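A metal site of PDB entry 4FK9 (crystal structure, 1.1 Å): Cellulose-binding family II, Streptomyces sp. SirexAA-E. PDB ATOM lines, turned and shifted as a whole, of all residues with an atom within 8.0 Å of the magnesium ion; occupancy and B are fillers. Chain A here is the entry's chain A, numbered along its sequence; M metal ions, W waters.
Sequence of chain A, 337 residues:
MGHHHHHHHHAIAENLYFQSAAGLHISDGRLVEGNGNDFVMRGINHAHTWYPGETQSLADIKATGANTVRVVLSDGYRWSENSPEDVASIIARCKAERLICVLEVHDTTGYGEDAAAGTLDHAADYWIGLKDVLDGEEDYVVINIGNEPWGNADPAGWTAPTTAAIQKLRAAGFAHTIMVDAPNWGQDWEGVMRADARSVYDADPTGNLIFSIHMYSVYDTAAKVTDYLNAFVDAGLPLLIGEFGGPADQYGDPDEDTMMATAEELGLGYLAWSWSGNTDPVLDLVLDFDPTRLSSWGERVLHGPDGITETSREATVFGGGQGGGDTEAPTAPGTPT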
ATOM      1  N   TYR A 216     -17.834 -22.160   9.253  1.00  0.00           N
ATOM      2  CA  TYR A 216     -18.290 -21.525  10.485  1.00  0.00           C
ATOM      3  C   TYR A 216     -19.328 -20.454  10.107  1.00  0.00           C
ATOM      4  O   TYR A 216     -20.165 -20.702   9.257  1.00  0.00           O
ATOM      5  CB  TYR A 216     -17.097 -21.042  11.315  1.00  0.00           C
ATOM      6  CG  TYR A 216     -16.250 -22.207  11.828  1.00  0.00           C
ATOM      7  CD1 TYR A 216     -16.598 -22.868  13.004  1.00  0.00           C
ATOM      8  CD2 TYR A 216     -15.146 -22.671  11.133  1.00  0.00           C
ATOM      9  CE1 TYR A 216     -15.853 -23.940  13.485  1.00  0.00           C
ATOM     10  CE2 TYR A 216     -14.387 -23.745  11.613  1.00  0.00           C
ATOM     11  CZ  TYR A 216     -14.757 -24.372  12.787  1.00  0.00           C
ATOM     12  OH  TYR A 216     -14.040 -25.420  13.304  1.00  0.00           O
ATOM     13  N   SER A 217     -19.290 -19.268  10.728  1.00  0.00           N
ATOM     14  CA  SER A 217     -20.415 -18.346  10.596  1.00  0.00           C
ATOM     15  C   SER A 217     -20.603 -17.676   9.231  1.00  0.00           C
ATOM     16  O   SER A 217     -21.625 -17.054   8.994  1.00  0.00           O
ATOM     17  CB  SER A 217     -20.391 -17.300  11.711  1.00  0.00           C
ATOM     18  OG  SER A 217     -20.699 -17.937  12.935  1.00  0.00           O
ATOM     19  N   TYR A 219     -21.138 -19.445   6.766  1.00  0.00           N
ATOM     20  CA  TYR A 219     -22.080 -20.368   6.163  1.00  0.00           C
ATOM     21  C   TYR A 219     -23.323 -20.496   7.034  1.00  0.00           C
ATOM     22  O   TYR A 219     -23.595 -21.534   7.630  1.00  0.00           O
ATOM     23  CB  TYR A 219     -21.382 -21.725   5.912  1.00  0.00           C
ATOM     24  CG  TYR A 219     -20.231 -21.504   4.964  1.00  0.00           C
ATOM     25  CD1 TYR A 219     -20.450 -21.471   3.601  1.00  0.00           C
ATOM     26  CD2 TYR A 219     -18.934 -21.233   5.426  1.00  0.00           C
ATOM     27  CE1 TYR A 219     -19.434 -21.204   2.717  1.00  0.00           C
ATOM     28  CE2 TYR A 219     -17.911 -20.965   4.547  1.00  0.00           C
ATOM     29  CZ  TYR A 219     -18.168 -20.946   3.185  1.00  0.00           C
ATOM     30  OH  TYR A 219     -17.198 -20.634   2.278  1.00  0.00           O
ATOM     31  N   ASP A 220     -24.062 -19.389   7.106  1.00  0.00           N
ATOM     32  CA  ASP A 220     -25.154 -19.244   8.062  1.00  0.00           C
ATOM     33  C   ASP A 220     -26.537 -19.322   7.417  1.00  0.00           C
ATOM     34  O   ASP A 220     -27.541 -19.070   8.078  1.00  0.00           O
ATOM     35  CB  ASP A 220     -24.993 -17.938   8.853  1.00  0.00           C
ATOM     36  CG  ASP A 220     -25.147 -16.697   7.993  1.00  0.00           C
ATOM     37  OD1 ASP A 220     -25.098 -16.776   6.756  1.00  0.00           O
ATOM     38  OD2 ASP A 220     -25.321 -15.608   8.578  1.00  0.00           O
ATOM     39  N   GLY A 245     -18.508 -25.939  12.448  1.00  0.00           N
ATOM     40  CA  GLY A 245     -19.185 -25.618  13.685  1.00  0.00           C
ATOM     41  C   GLY A 245     -20.691 -25.655  13.517  1.00  0.00           C
ATOM     42  O   GLY A 245     -21.224 -26.255  12.578  1.00  0.00           O
ATOM     43  N   GLY A 246     -21.405 -24.994  14.427  1.00  0.00           N
ATOM     44  CA  GLY A 246     -22.838 -25.153  14.474  1.00  0.00           C
ATOM     45  C   GLY A 246     -23.470 -24.175  15.427  1.00  0.00           C
ATOM     46  O   GLY A 246     -24.317 -23.379  15.029  1.00  0.00           O
ATOM     47  N   PRO A 247     -23.077 -24.234  16.710  1.00  0.00           N
ATOM     48  CA  PRO A 247     -23.649 -23.286  17.667  1.00  0.00           C
ATOM     49  C   PRO A 247     -23.328 -21.828  17.275  1.00  0.00           C
ATOM     50  O   PRO A 247     -22.266 -21.534  16.743  1.00  0.00           O
ATOM     51  CB  PRO A 247     -22.976 -23.676  18.991  1.00  0.00           C
ATOM     52  CG  PRO A 247     -22.594 -25.129  18.807  1.00  0.00           C
ATOM     53  CD  PRO A 247     -22.219 -25.237  17.358  1.00  0.00           C
ATOM     54  N   ALA A 248     -24.266 -20.919  17.524  1.00  0.00           N
ATOM     55  CA  ALA A 248     -24.033 -19.529  17.181  1.00  0.00           C
ATOM     56  C   ALA A 248     -22.833 -18.969  17.938  1.00  0.00           C
ATOM     57  O   ALA A 248     -22.611 -19.307  19.096  1.00  0.00           O
ATOM     58  CB  ALA A 248     -25.272 -18.702  17.478  1.00  0.00           C
ATOM     59  N   ASP A 249     -22.046 -18.141  17.259  1.00  0.00           N
ATOM     60  CA  ASP A 249     -20.972 -17.377  17.901  1.00  0.00           C
ATOM     61  C   ASP A 249     -21.212 -15.882  17.669  1.00  0.00           C
ATOM     62  O   ASP A 249     -22.287 -15.480  17.235  1.00  0.00           O
ATOM     63  CB  ASP A 249     -19.577 -17.830  17.437  1.00  0.00           C
ATOM     64  CG  ASP A 249     -19.344 -17.633  15.944  1.00  0.00           C
ATOM     65  OD1 ASP A 249     -20.054 -16.842  15.299  1.00  0.00           O
ATOM     66  OD2 ASP A 249     -18.399 -18.264  15.408  1.00  0.00           O
ATOM     67  N   GLY A 252     -22.237 -15.040  13.890  1.00  0.00           N
ATOM     68  CA  GLY A 252     -23.418 -15.569  13.241  1.00  0.00           C
ATOM     69  C   GLY A 252     -23.717 -16.970  13.720  1.00  0.00           C
ATOM     70  O   GLY A 252     -23.185 -17.413  14.734  1.00  0.00           O
ATOM     71  N   ASP A 253     -24.573 -17.676  12.989  1.00  0.00           N
ATOM     72  CA  ASP A 253     -24.970 -19.031  13.366  1.00  0.00           C
ATOM     73  C   ASP A 253     -24.707 -19.991  12.204  1.00  0.00           C
ATOM     74  O   ASP A 253     -25.492 -20.021  11.254  1.00  0.00           O
ATOM     75  CB  ASP A 253     -26.455 -19.067  13.748  1.00  0.00           C
ATOM     76  CG  ASP A 253     -26.894 -20.409  14.296  1.00  0.00           C
ATOM     77  OD1 ASP A 253     -26.169 -21.403  14.110  1.00  0.00           O
ATOM     78  OD2 ASP A 253     -27.979 -20.470  14.926  1.00  0.00           O
ATOM     79  N   PRO A 254     -23.611 -20.758  12.261  1.00  0.00           N
ATOM     80  CA  PRO A 254     -23.355 -21.722  11.174  1.00  0.00           C
ATOM     81  C   PRO A 254     -24.539 -22.672  11.020  1.00  0.00           C
ATOM     82  O   PRO A 254     -25.086 -23.131  12.014  1.00  0.00           O
ATOM     83  CB  PRO A 254     -22.107 -22.478  11.641  1.00  0.00           C
ATOM     84  CG  PRO A 254     -21.471 -21.588  12.662  1.00  0.00           C
ATOM     85  CD  PRO A 254     -22.619 -20.893  13.334  1.00  0.00           C
ATOM     86  N   ASP A 255     -24.923 -22.959   9.772  1.00  0.00           N
ATOM     87  CA  ASP A 255     -26.051 -23.835   9.480  1.00  0.00           C
ATOM     88  C   ASP A 255     -25.611 -25.301   9.384  1.00  0.00           C
ATOM     89  O   ASP A 255     -25.466 -25.872   8.298  1.00  0.00           O
ATOM     90  CB  ASP A 255     -26.736 -23.375   8.188  1.00  0.00           C
ATOM     91  CG  ASP A 255     -27.961 -24.187   7.825  1.00  0.00           C
ATOM     92  OD1 ASP A 255     -28.372 -25.079   8.604  1.00  0.00           O
ATOM     93  OD2 ASP A 255     -28.521 -23.920   6.747  1.00  0.00           O
ATOM     94  N   GLU A 256     -25.378 -25.910  10.541  1.00  0.00           N
ATOM     95  CA  GLU A 256     -24.877 -27.270  10.598  1.00  0.00           C
ATOM     96  C   GLU A 256     -25.852 -28.276   9.971  1.00  0.00           C
ATOM     97  O   GLU A 256     -25.426 -29.264   9.386  1.00  0.00           O
ATOM     98  CB  GLU A 256     -24.521 -27.683  12.041  1.00  0.00           C
ATOM     99  CG  GLU A 256     -25.688 -27.861  13.026  1.00  0.00           C
ATOM    100  CD  GLU A 256     -26.114 -26.585  13.746  1.00  0.00           C
ATOM    101  OE1 GLU A 256     -25.749 -25.466  13.309  1.00  0.00           O
ATOM    102  OE2 GLU A 256     -26.831 -26.701  14.752  1.00  0.00           O
ATOM    103  N   ASP A 257     -27.160 -28.019  10.074  1.00  0.00           N
ATOM    104  CA  ASP A 257     -28.128 -28.958   9.520  1.00  0.00           C
ATOM    105  C   ASP A 257     -27.949 -29.107   8.014  1.00  0.00           C
ATOM    106  O   ASP A 257     -27.909 -30.220   7.506  1.00  0.00           O
ATOM    107  CB  ASP A 257     -29.562 -28.509   9.839  1.00  0.00           C
ATOM    108  CG  ASP A 257     -29.882 -28.581  11.314  1.00  0.00           C
ATOM    109  OD1 ASP A 257     -29.436 -29.517  11.991  1.00  0.00           O
ATOM    110  OD2 ASP A 257     -30.599 -27.696  11.817  1.00  0.00           O
ATOM    111  N   MET A 259     -25.266 -28.302   6.282  1.00  0.00           N
ATOM    112  CA  MET A 259     -23.941 -28.849   6.006  1.00  0.00           C
ATOM    113  C   MET A 259     -23.999 -30.371   6.020  1.00  0.00           C
ATOM    114  O   MET A 259     -23.504 -31.028   5.100  1.00  0.00           O
ATOM    115  CB  MET A 259     -22.928 -28.380   7.057  1.00  0.00           C
ATOM    116  CG  MET A 259     -22.639 -26.899   7.037  1.00  0.00           C
ATOM    117  SD  MET A 259     -21.577 -26.492   8.419  1.00  0.00           S
ATOM    118  CE  MET A 259     -21.873 -24.737   8.576  1.00  0.00           C
ATOM    119  N   TRP A 297     -23.657 -29.975  21.463  1.00  0.00           N
ATOM    120  CA  TRP A 297     -23.036 -30.095  20.153  1.00  0.00           C
ATOM    121  C   TRP A 297     -22.633 -31.555  19.858  1.00  0.00           C
ATOM    122  O   TRP A 297     -22.859 -32.047  18.749  1.00  0.00           O
ATOM    123  CB  TRP A 297     -21.855 -29.130  20.129  1.00  0.00           C
ATOM    124  CG  TRP A 297     -20.916 -29.173  18.995  1.00  0.00           C
ATOM    125  CD1 TRP A 297     -19.571 -29.265  19.110  1.00  0.00           C
ATOM    126  CD2 TRP A 297     -21.191 -29.035  17.592  1.00  0.00           C
ATOM    127  NE1 TRP A 297     -18.976 -29.196  17.884  1.00  0.00           N
ATOM    128  CE2 TRP A 297     -19.947 -29.069  16.933  1.00  0.00           C
ATOM    129  CE3 TRP A 297     -22.356 -28.897  16.828  1.00  0.00           C
ATOM    130  CZ2 TRP A 297     -19.820 -28.972  15.563  1.00  0.00           C
ATOM    131  CZ3 TRP A 297     -22.221 -28.793  15.448  1.00  0.00           C
ATOM    132  CH2 TRP A 297     -20.969 -28.841  14.827  1.00  0.00           C
HETATM  133 MG    MG M   1     -26.022 -23.414  13.850  1.00  0.00          MG
HETATM  134  O   HOH W   1     -27.102 -24.056  15.493  1.00  0.00           O
HETATM  135  O   HOH W   2     -27.860 -23.389  12.797  1.00  0.00           O
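Within 4 Å of the magnesium ion: Gly 246, Asp 253, Pro 254 and Glu 256.
Along chain A the residues within 4 Å of the magnesium ion span positions 246 to 256.
The nearest printed residue that does not touch the magnesium ion is Pro 247 (4.2 Å).
The magnesium ion is bound by the side-chain carboxylate (OD1) of Asp 253 (2.0 Å), water W1 (2.1 Å), the backbone carbonyl oxygen (O) of Gly 246 (2.1 Å), the backbone carbonyl oxygen (O) of Pro 254 (2.1 Å), water W2 (2.1 Å) and the side-chain carboxylate (OE1) of Glu 256 (2.1 Å).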
